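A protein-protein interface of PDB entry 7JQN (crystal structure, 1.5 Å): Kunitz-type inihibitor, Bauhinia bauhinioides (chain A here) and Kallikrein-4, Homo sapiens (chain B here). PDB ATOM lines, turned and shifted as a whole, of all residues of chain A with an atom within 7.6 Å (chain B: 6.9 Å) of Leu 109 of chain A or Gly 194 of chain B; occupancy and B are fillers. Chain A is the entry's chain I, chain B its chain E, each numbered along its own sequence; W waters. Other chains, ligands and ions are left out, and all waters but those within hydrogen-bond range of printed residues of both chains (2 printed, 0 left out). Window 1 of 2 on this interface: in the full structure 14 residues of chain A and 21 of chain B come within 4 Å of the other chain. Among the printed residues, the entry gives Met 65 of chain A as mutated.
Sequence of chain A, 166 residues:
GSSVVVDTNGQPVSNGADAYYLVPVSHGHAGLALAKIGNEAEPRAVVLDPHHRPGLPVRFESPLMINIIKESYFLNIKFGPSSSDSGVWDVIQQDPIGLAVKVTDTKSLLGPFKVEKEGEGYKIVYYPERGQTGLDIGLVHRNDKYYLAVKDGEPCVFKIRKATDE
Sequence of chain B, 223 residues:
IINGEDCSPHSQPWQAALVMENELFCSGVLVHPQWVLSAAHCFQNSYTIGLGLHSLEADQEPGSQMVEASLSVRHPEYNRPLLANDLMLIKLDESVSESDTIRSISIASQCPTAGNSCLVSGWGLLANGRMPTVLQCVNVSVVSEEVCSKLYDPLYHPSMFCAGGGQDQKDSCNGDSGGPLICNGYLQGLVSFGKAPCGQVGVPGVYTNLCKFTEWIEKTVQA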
ATOM      1  N   GLU A  61     -33.111 -19.304 -33.772  1.00  0.00           N
ATOM      2  CA  GLU A  61     -32.619 -19.373 -32.394  1.00  0.00           C
ATOM      3  C   GLU A  61     -31.339 -18.546 -32.253  1.00  0.00           C
ATOM      4  O   GLU A  61     -30.396 -18.672 -33.040  1.00  0.00           O
ATOM      5  CB  GLU A  61     -32.319 -20.838 -32.004  1.00  0.00           C
ATOM      6  CG  GLU A  61     -33.575 -21.720 -31.916  1.00  0.00           C
ATOM      7  CD  GLU A  61     -33.310 -23.163 -31.508  1.00  0.00           C
ATOM      8  OE1 GLU A  61     -32.224 -23.675 -31.827  1.00  0.00           O
ATOM      9  OE2 GLU A  61     -34.182 -23.758 -30.856  1.00  0.00           O
ATOM     10  N   SER A  62     -31.285 -17.752 -31.183  1.00  0.00           N
ATOM     11  CA  SER A  62     -30.084 -17.052 -30.742  1.00  0.00           C
ATOM     12  C   SER A  62     -29.856 -17.416 -29.275  1.00  0.00           C
ATOM     13  O   SER A  62     -30.813 -17.583 -28.525  1.00  0.00           O
ATOM     14  CB  SER A  62     -30.341 -15.552 -30.838  1.00  0.00           C
ATOM     15  OG  SER A  62     -29.405 -14.793 -30.066  1.00  0.00           O
ATOM     16  N   PRO A  63     -28.593 -17.534 -28.813  1.00  0.00           N
ATOM     17  CA  PRO A  63     -28.329 -17.806 -27.405  1.00  0.00           C
ATOM     18  C   PRO A  63     -28.620 -16.639 -26.480  1.00  0.00           C
ATOM     19  O   PRO A  63     -28.687 -16.836 -25.275  1.00  0.00           O
ATOM     20  CB  PRO A  63     -26.828 -18.163 -27.407  1.00  0.00           C
ATOM     21  CG  PRO A  63     -26.249 -17.340 -28.554  1.00  0.00           C
ATOM     22  CD  PRO A  63     -27.349 -17.393 -29.616  1.00  0.00           C
ATOM     23  N   LEU A  64     -28.844 -15.436 -27.052  1.00  0.00           N
ATOM     24  CA  LEU A  64     -29.128 -14.270 -26.220  1.00  0.00           C
ATOM     25  C   LEU A  64     -30.431 -14.499 -25.443  1.00  0.00           C
ATOM     26  O   LEU A  64     -31.377 -15.085 -25.979  1.00  0.00           O
ATOM     27  CB  LEU A  64     -29.253 -13.027 -27.123  1.00  0.00           C
ATOM     28  CG  LEU A  64     -27.984 -12.706 -27.951  1.00  0.00           C
ATOM     29  CD1 LEU A  64     -28.306 -11.648 -29.024  1.00  0.00           C
ATOM     30  CD2 LEU A  64     -26.825 -12.239 -27.038  1.00  0.00           C
ATOM     31  N   MET A  65     -30.497 -13.960 -24.215  1.00  0.00           N
ATOM     32  CA  MET A  65     -31.617 -14.210 -23.309  1.00  0.00           C
ATOM     33  C   MET A  65     -32.800 -13.282 -23.599  1.00  0.00           C
ATOM     34  O   MET A  65     -33.461 -12.770 -22.682  1.00  0.00           O
ATOM     35  CB  MET A  65     -31.181 -14.032 -21.852  1.00  0.00           C
ATOM     36  CG  MET A  65     -30.712 -15.318 -21.199  1.00  0.00           C
ATOM     37  SD  MET A  65     -31.699 -16.821 -21.447  1.00  0.00           S
ATOM     38  CE  MET A  65     -30.726 -17.687 -22.675  1.00  0.00           C
ATOM     39  N   PHE A  74     -26.637 -13.400 -35.090  1.00  0.00           N
ATOM     40  CA  PHE A  74     -26.355 -14.709 -35.674  1.00  0.00           C
ATOM     41  C   PHE A  74     -27.366 -15.722 -35.142  1.00  0.00           C
ATOM     42  O   PHE A  74     -27.615 -15.805 -33.924  1.00  0.00           O
ATOM     43  CB  PHE A  74     -24.953 -15.184 -35.285  1.00  0.00           C
ATOM     44  CG  PHE A  74     -23.874 -14.664 -36.200  1.00  0.00           C
ATOM     45  CD1 PHE A  74     -23.886 -15.021 -37.553  1.00  0.00           C
ATOM     46  CD2 PHE A  74     -22.841 -13.841 -35.723  1.00  0.00           C
ATOM     47  CE1 PHE A  74     -22.907 -14.544 -38.411  1.00  0.00           C
ATOM     48  CE2 PHE A  74     -21.843 -13.387 -36.583  1.00  0.00           C
ATOM     49  CZ  PHE A  74     -21.886 -13.760 -37.916  1.00  0.00           C
ATOM     50  N   LEU A  75     -27.906 -16.527 -36.070  1.00  0.00           N
ATOM     51  CA  LEU A  75     -29.008 -17.436 -35.777  1.00  0.00           C
ATOM     52  C   LEU A  75     -28.655 -18.857 -36.196  1.00  0.00           C
ATOM     53  O   LEU A  75     -27.992 -19.082 -37.235  1.00  0.00           O
ATOM     54  CB  LEU A  75     -30.245 -17.008 -36.595  1.00  0.00           C
ATOM     55  CG  LEU A  75     -30.726 -15.590 -36.328  1.00  0.00           C
ATOM     56  CD1 LEU A  75     -31.889 -15.288 -37.286  1.00  0.00           C
ATOM     57  CD2 LEU A  75     -31.179 -15.449 -34.873  1.00  0.00           C
ATOM     58  N   ASN A  76     -29.196 -19.808 -35.418  1.00  0.00           N
ATOM     59  CA  ASN A  76     -29.487 -21.136 -35.951  1.00  0.00           C
ATOM     60  C   ASN A  76     -30.887 -21.107 -36.564  1.00  0.00           C
ATOM     61  O   ASN A  76     -31.769 -20.381 -36.090  1.00  0.00           O
ATOM     62  CB  ASN A  76     -29.423 -22.214 -34.858  1.00  0.00           C
ATOM     63  CG  ASN A  76     -28.000 -22.628 -34.559  1.00  0.00           C
ATOM     64  OD1 ASN A  76     -27.328 -23.098 -35.468  1.00  0.00           O
ATOM     65  ND2 ASN A  76     -27.532 -22.403 -33.329  1.00  0.00           N
ATOM     66  N   LYS A 107     -25.669 -28.781 -33.373  1.00  0.00           N
ATOM     67  CA  LYS A 107     -25.958 -27.368 -33.351  1.00  0.00           C
ATOM     68  C   LYS A 107     -24.852 -26.682 -32.562  1.00  0.00           C
ATOM     69  O   LYS A 107     -24.542 -27.097 -31.452  1.00  0.00           O
ATOM     70  CB  LYS A 107     -27.269 -27.206 -32.575  1.00  0.00           C
ATOM     71  CG  LYS A 107     -27.793 -25.792 -32.416  1.00  0.00           C
ATOM     72  CD  LYS A 107     -28.712 -25.667 -31.226  1.00  0.00           C
ATOM     73  CE  LYS A 107     -30.161 -25.843 -31.584  1.00  0.00           C
ATOM     74  NZ  LYS A 107     -31.009 -25.753 -30.371  1.00  0.00           N
ATOM     75  N   SER A 108     -24.274 -25.632 -33.132  1.00  0.00           N
ATOM     76  CA  SER A 108     -23.379 -24.761 -32.388  1.00  0.00           C
ATOM     77  C   SER A 108     -24.191 -23.805 -31.517  1.00  0.00           C
ATOM     78  O   SER A 108     -25.333 -23.483 -31.837  1.00  0.00           O
ATOM     79  CB  SER A 108     -22.435 -24.011 -33.327  1.00  0.00           C
ATOM     80  OG  SER A 108     -21.600 -24.908 -34.077  1.00  0.00           O
ATOM     81  N   LEU A 109     -23.580 -23.278 -30.461  1.00  0.00           N
ATOM     82  CA  LEU A 109     -24.237 -22.295 -29.614  1.00  0.00           C
ATOM     83  C   LEU A 109     -24.697 -21.103 -30.449  1.00  0.00           C
ATOM     84  O   LEU A 109     -25.771 -20.534 -30.215  1.00  0.00           O
ATOM     85  CB  LEU A 109     -23.276 -21.849 -28.493  1.00  0.00           C
ATOM     86  CG  LEU A 109     -23.856 -20.844 -27.499  1.00  0.00           C
ATOM     87  CD1 LEU A 109     -24.979 -21.459 -26.673  1.00  0.00           C
ATOM     88  CD2 LEU A 109     -22.765 -20.288 -26.581  1.00  0.00           C
ATOM     89  N   LEU A 110     -23.842 -20.695 -31.381  1.00  0.00           N
ATOM     90  CA  LEU A 110     -24.113 -19.552 -32.221  1.00  0.00           C
ATOM     91  C   LEU A 110     -24.138 -20.036 -33.666  1.00  0.00           C
ATOM     92  O   LEU A 110     -23.159 -20.588 -34.171  1.00  0.00           O
ATOM     93  CB  LEU A 110     -22.954 -18.595 -31.937  1.00  0.00           C
ATOM     94  CG  LEU A 110     -23.145 -17.157 -32.357  1.00  0.00           C
ATOM     95  CD1 LEU A 110     -24.410 -16.556 -31.737  1.00  0.00           C
ATOM     96  CD2 LEU A 110     -21.912 -16.367 -31.961  1.00  0.00           C
ATOM     97  N   GLY A 111     -25.281 -19.861 -34.338  1.00  0.00           N
ATOM     98  CA  GLY A 111     -25.403 -20.360 -35.702  1.00  0.00           C
ATOM     99  C   GLY A 111     -24.798 -19.384 -36.712  1.00  0.00           C
ATOM    100  O   GLY A 111     -24.349 -18.293 -36.348  1.00  0.00           O
ATOM    101  N   ARG A 130     -18.777 -17.456 -39.258  1.00  0.00           N
ATOM    102  CA  ARG A 130     -19.385 -16.363 -38.493  1.00  0.00           C
ATOM    103  C   ARG A 130     -18.490 -15.123 -38.574  1.00  0.00           C
ATOM    104  O   ARG A 130     -18.326 -14.376 -37.596  1.00  0.00           O
ATOM    105  CB  ARG A 130     -19.647 -16.751 -37.032  1.00  0.00           C
ATOM    106  CG  ARG A 130     -20.747 -17.791 -36.845  1.00  0.00           C
ATOM    107  CD  ARG A 130     -20.505 -19.145 -37.473  1.00  0.00           C
ATOM    108  NE  ARG A 130     -21.360 -20.133 -36.809  1.00  0.00           N
ATOM    109  CZ  ARG A 130     -21.454 -21.406 -37.153  1.00  0.00           C
ATOM    110  NH1 ARG A 130     -22.258 -22.195 -36.465  1.00  0.00           N
ATOM    111  NH2 ARG A 130     -20.697 -21.901 -38.136  1.00  0.00           N
ATOM    112  N   LEU B  83     -20.361 -12.057 -28.888  1.00  0.00           N
ATOM    113  CA  LEU B  83     -21.136 -12.104 -27.635  1.00  0.00           C
ATOM    114  C   LEU B  83     -20.482 -11.332 -26.486  1.00  0.00           C
ATOM    115  O   LEU B  83     -21.148 -11.118 -25.459  1.00  0.00           O
ATOM    116  CB  LEU B  83     -21.463 -13.531 -27.163  1.00  0.00           C
ATOM    117  CG  LEU B  83     -22.171 -14.417 -28.190  1.00  0.00           C
ATOM    118  CD1 LEU B  83     -22.376 -15.814 -27.639  1.00  0.00           C
ATOM    119  CD2 LEU B  83     -23.528 -13.817 -28.574  1.00  0.00           C
ATOM    120  N   LEU B 151     -16.884 -24.882 -20.295  1.00  0.00           N
ATOM    121  CA  LEU B 151     -18.187 -25.085 -20.926  1.00  0.00           C
ATOM    122  C   LEU B 151     -18.354 -24.204 -22.174  1.00  0.00           C
ATOM    123  O   LEU B 151     -19.036 -24.608 -23.129  1.00  0.00           O
ATOM    124  CB  LEU B 151     -19.279 -24.792 -19.885  1.00  0.00           C
ATOM    125  CG  LEU B 151     -19.279 -25.742 -18.677  1.00  0.00           C
ATOM    126  CD1 LEU B 151     -20.360 -25.345 -17.680  1.00  0.00           C
ATOM    127  CD2 LEU B 151     -19.403 -27.207 -19.092  1.00  0.00           C
ATOM    128  N   TYR B 152     -17.785 -22.981 -22.160  1.00  0.00           N
ATOM    129  CA  TYR B 152     -18.170 -21.995 -23.180  1.00  0.00           C
ATOM    130  C   TYR B 152     -17.052 -21.614 -24.150  1.00  0.00           C
ATOM    131  O   TYR B 152     -17.370 -21.027 -25.182  1.00  0.00           O
ATOM    132  CB  TYR B 152     -18.762 -20.725 -22.556  1.00  0.00           C
ATOM    133  CG  TYR B 152     -20.195 -20.889 -22.109  1.00  0.00           C
ATOM    134  CD1 TYR B 152     -21.233 -20.841 -23.037  1.00  0.00           C
ATOM    135  CD2 TYR B 152     -20.517 -21.103 -20.763  1.00  0.00           C
ATOM    136  CE1 TYR B 152     -22.557 -20.988 -22.642  1.00  0.00           C
ATOM    137  CE2 TYR B 152     -21.836 -21.284 -20.363  1.00  0.00           C
ATOM    138  CZ  TYR B 152     -22.866 -21.203 -21.302  1.00  0.00           C
ATOM    139  OH  TYR B 152     -24.188 -21.341 -20.935  1.00  0.00           O
ATOM    140  N   LEU B 155     -16.058 -19.221 -26.869  1.00  0.00           N
ATOM    141  CA  LEU B 155     -16.791 -17.958 -26.768  1.00  0.00           C
ATOM    142  C   LEU B 155     -16.703 -17.342 -25.371  1.00  0.00           C
ATOM    143  O   LEU B 155     -17.252 -16.269 -25.153  1.00  0.00           O
ATOM    144  CB  LEU B 155     -18.243 -18.177 -27.198  1.00  0.00           C
ATOM    145  CG  LEU B 155     -18.434 -18.498 -28.674  1.00  0.00           C
ATOM    146  CD1 LEU B 155     -19.899 -18.807 -28.972  1.00  0.00           C
ATOM    147  CD2 LEU B 155     -17.934 -17.332 -29.536  1.00  0.00           C
ATOM    148  N   SER B 192     -27.140 -12.043 -20.006  1.00  0.00           N
ATOM    149  CA  SER B 192     -26.624 -11.876 -21.369  1.00  0.00           C
ATOM    150  C   SER B 192     -27.046 -13.036 -22.279  1.00  0.00           C
ATOM    151  O   SER B 192     -27.860 -12.840 -23.187  1.00  0.00           O
ATOM    152  CB  SER B 192     -25.101 -11.668 -21.356  1.00  0.00           C
ATOM    153  OG  SER B 192     -24.564 -11.555 -22.681  1.00  0.00           O
ATOM    154  N   PHE B 193     -26.529 -14.260 -22.069  1.00  0.00           N
ATOM    155  CA  PHE B 193     -26.824 -15.347 -23.015  1.00  0.00           C
ATOM    156  C   PHE B 193     -26.687 -16.696 -22.320  1.00  0.00           C
ATOM    157  O   PHE B 193     -26.269 -16.764 -21.158  1.00  0.00           O
ATOM    158  CB  PHE B 193     -25.946 -15.293 -24.291  1.00  0.00           C
ATOM    159  CG  PHE B 193     -24.480 -15.642 -24.087  1.00  0.00           C
ATOM    160  CD1 PHE B 193     -23.552 -14.657 -23.768  1.00  0.00           C
ATOM    161  CD2 PHE B 193     -24.024 -16.941 -24.310  1.00  0.00           C
ATOM    162  CE1 PHE B 193     -22.197 -14.977 -23.610  1.00  0.00           C
ATOM    163  CE2 PHE B 193     -22.676 -17.273 -24.135  1.00  0.00           C
ATOM    164  CZ  PHE B 193     -21.761 -16.288 -23.814  1.00  0.00           C
ATOM    165  N   GLY B 194     -27.064 -17.776 -23.010  1.00  0.00           N
ATOM    166  CA  GLY B 194     -26.886 -19.097 -22.423  1.00  0.00           C
ATOM    167  C   GLY B 194     -27.246 -20.189 -23.423  1.00  0.00           C
ATOM    168  O   GLY B 194     -27.600 -19.900 -24.559  1.00  0.00           O
ATOM    169  N   LYS B 195     -27.118 -21.436 -22.983  1.00  0.00           N
ATOM    170  CA  LYS B 195     -27.432 -22.617 -23.778  1.00  0.00           C
ATOM    171  C   LYS B 195     -28.898 -23.009 -23.577  1.00  0.00           C
ATOM    172  O   LYS B 195     -29.332 -23.178 -22.448  1.00  0.00           O
ATOM    173  CB  LYS B 195     -26.538 -23.776 -23.322  1.00  0.00           C
ATOM    174  CG  LYS B 195     -25.038 -23.594 -23.549  1.00  0.00           C
ATOM    175  CD  LYS B 195     -24.168 -24.793 -23.151  1.00  0.00           C
ATOM    176  CE  LYS B 195     -22.682 -24.532 -23.316  1.00  0.00           C
ATOM    177  NZ  LYS B 195     -21.878 -25.755 -23.120  1.00  0.00           N
ATOM    178  N   ALA B 196     -29.670 -23.179 -24.660  1.00  0.00           N
ATOM    179  CA  ALA B 196     -31.083 -23.514 -24.509  1.00  0.00           C
ATOM    180  C   ALA B 196     -31.234 -25.028 -24.391  1.00  0.00           C
ATOM    181  O   ALA B 196     -30.416 -25.775 -24.943  1.00  0.00           O
ATOM    182  CB  ALA B 196     -31.846 -22.992 -25.706  1.00  0.00           C
ATOM    183  N   PRO B 197     -32.257 -25.557 -23.672  1.00  0.00           N
ATOM    184  CA  PRO B 197     -33.220 -24.751 -22.914  1.00  0.00           C
ATOM    185  C   PRO B 197     -32.684 -24.227 -21.575  1.00  0.00           C
ATOM    186  O   PRO B 197     -31.675 -24.698 -21.049  1.00  0.00           O
ATOM    187  CB  PRO B 197     -34.337 -25.777 -22.639  1.00  0.00           C
ATOM    188  CG  PRO B 197     -33.606 -27.101 -22.521  1.00  0.00           C
ATOM    189  CD  PRO B 197     -32.513 -27.002 -23.554  1.00  0.00           C
ATOM    190  N   CSO B 198     -33.398 -23.253 -20.997  1.00  0.00           N
ATOM    191  CA  CSO B 198     -33.072 -22.705 -19.685  1.00  0.00           C
ATOM    192  CB  CSO B 198     -34.035 -21.555 -19.371  1.00  0.00           C
ATOM    193  SG  CSO B 198     -34.099 -20.315 -20.690  1.00  0.00           S
ATOM    194  C   CSO B 198     -33.253 -23.771 -18.606  1.00  0.00           C
ATOM    195  O   CSO B 198     -34.060 -24.683 -18.764  1.00  0.00           O
ATOM    196  OD  CSO B 198     -32.485 -20.068 -20.766  1.00  0.00           O
ATOM    197  N   VAL B 203     -25.612 -26.608 -16.409  1.00  0.00           N
ATOM    198  CA  VAL B 203     -25.396 -25.628 -17.465  1.00  0.00           C
ATOM    199  C   VAL B 203     -25.695 -24.245 -16.885  1.00  0.00           C
ATOM    200  O   VAL B 203     -26.848 -23.868 -16.682  1.00  0.00           O
ATOM    201  CB  VAL B 203     -26.299 -25.901 -18.687  1.00  0.00           C
ATOM    202  CG1 VAL B 203     -26.032 -24.898 -19.812  1.00  0.00           C
ATOM    203  CG2 VAL B 203     -26.156 -27.344 -19.191  1.00  0.00           C
ATOM    204  N   PRO B 204     -24.674 -23.440 -16.554  1.00  0.00           N
ATOM    205  CA  PRO B 204     -24.918 -22.098 -16.035  1.00  0.00           C
ATOM    206  C   PRO B 204     -25.221 -21.149 -17.191  1.00  0.00           C
ATOM    207  O   PRO B 204     -24.872 -21.407 -18.346  1.00  0.00           O
ATOM    208  CB  PRO B 204     -23.592 -21.718 -15.366  1.00  0.00           C
ATOM    209  CG  PRO B 204     -22.535 -22.564 -16.071  1.00  0.00           C
ATOM    210  CD  PRO B 204     -23.249 -23.776 -16.638  1.00  0.00           C
ATOM    211  N   GLY B 205     -25.872 -20.041 -16.839  1.00  0.00           N
ATOM    212  CA  GLY B 205     -26.083 -18.941 -17.769  1.00  0.00           C
ATOM    213  C   GLY B 205     -24.889 -17.984 -17.745  1.00  0.00           C
ATOM    214  O   GLY B 205     -24.046 -18.049 -16.832  1.00  0.00           O
ATOM    215  N   VAL B 206     -24.783 -17.113 -18.752  1.00  0.00           N
ATOM    216  CA  VAL B 206     -23.658 -16.189 -18.882  1.00  0.00           C
ATOM    217  C   VAL B 206     -24.143 -14.746 -18.714  1.00  0.00           C
ATOM    218  O   VAL B 206     -25.192 -14.335 -19.249  1.00  0.00           O
ATOM    219  CB  VAL B 206     -22.918 -16.400 -20.220  1.00  0.00           C
ATOM    220  CG1 VAL B 206     -21.652 -15.532 -20.252  1.00  0.00           C
ATOM    221  CG2 VAL B 206     -22.571 -17.884 -20.424  1.00  0.00           C
HETATM  222  O   HOH W   1     -29.396 -25.445 -27.569  1.00  0.00           O
HETATM  223  O   HOH W   2     -30.233 -19.292 -19.123  1.00  0.00           O
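Pro 63 of chain A touches Phe 193 of chain B (O to CA, 3.3 Å).
Leu 64 of chain A touches Leu 83 of chain B.
Ser 192 of chain B touches Leu 64 of chain A (O to CA, 3.6 Å).
Leu 64 of chain A touches Phe 193 of chain B.
Met 65 of chain A touches Gly 194 of chain B (CE to N, 3.7 Å).
Tyr 152 of chain B touches Leu 109 of chain A.
Leu 109 of chain A touches Phe 193 of chain B (CD2 to CE2, 3.9 Å).
CD1 of Leu 109 of chain A touches O of Gly 194 of chain B, 3.7 Å away.
CG of Lys 195 of chain B touches CD1 of Leu 109 of chain A (3.8 Å).
Of the printed residues of chain B, Leu 109 of chain A touches Tyr 152 (3.9 Å), Phe 193 (3.9 Å), Gly 194 (3.7 Å) and Lys 195 (3.8 Å).
Printed residues of chain A within 4 Å of Gly 194 of chain B: Pro 63 (2.9 Å), Met 65 (3.7 Å) and Leu 109 (3.7 Å).
Of the printed residues of chain B, Leu 64 of chain A touches Leu 83, Ser 192 and Phe 193.
Of the printed residues of chain A, Phe 193 of chain B touches Pro 63, Leu 64 and Leu 109.
Of the printed residues of chain B, Met 65 of chain A touches Ser 192 (3.0 Å), Gly 194 (3.7 Å) and CSO 198 (3.4 Å).
Of the printed residues of chain A, Lys 195 of chain B touches Leu 109.
Of the printed residues of chain A, Ser 192 of chain B touches Leu 64 (3.6 Å) and Met 65 (3.0 Å).
Pro 197 of chain B touches none of the printed residues of chain A.
Leu 110 of chain A touches none of the printed residues of chain B.
The nearest printed residue of chain A that does not touch Gly 194 of chain B is Leu 64 of chain A (5.0 Å).
Water W1 lies within hydrogen-bond range of the backbone carbonyl oxygen of Ala 196 of chain B and the side-chain amino group of Lys 107 of chain A.
Water W2 lies within hydrogen-bond range of OD of CSO 198 of chain B (2.9 Å) and SD of Met 65 of chain A (3.7 Å).
Printed residues of chain B that touch a printed residue of chain A: Leu 83, Tyr 152, Ser 192, Phe 193, Gly 194, Lys 195 and CSO 198.
Hydrophobic or aromatic side chains of chain B that line the printed part of chain A: Leu 83, Tyr 152 and Phe 193.
Along chain B the printed residues that touch a printed residue of chain A span positions 83 to 198.
Of the 14 printed residues of chain A, 4 touch a printed residue of chain B.
Hydrophobic or aromatic side chains of chain A within 4 Å of the printed part of chain B: Pro 63, Leu 64, Met 65 and Leu 109.
Among the printed residues, 12 pairs touch across the chains.
The side-chain amino group (NZ) of Lys 195 of chain B is in hydrogen-bond range of the backbone carbonyl oxygen (O) of Leu 151 of chain B (3.1 Å).
OH of Tyr 152 of chain B is in hydrogen-bond range of O of Pro 204 of chain B, at 2.7 Å.
O of Val 206 of chain B is in hydrogen-bond range of N of Ser 192 of chain B (3.1 Å).
O of Phe 193 of chain B lies within hydrogen-bond range of N of Val 206 of chain B (2.8 Å).
The side-chain hydroxyl (OG) of Ser 62 of chain A is in hydrogen-bond range of the backbone NH (N) of Leu 64 of chain A.
The backbone carbonyl oxygen (O) of Ser 192 of chain B sits at hydrogen-bond distance from the backbone NH (N) of Met 65 of chain A, at 3.0 Å.
N of Gly 194 of chain B lies within hydrogen-bond range of O of Pro 63 of chain A, at 2.9 Å.
OD of CSO 198 of chain B lies within hydrogen-bond range of SD of Met 65 of chain A, 3.4 Å away.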
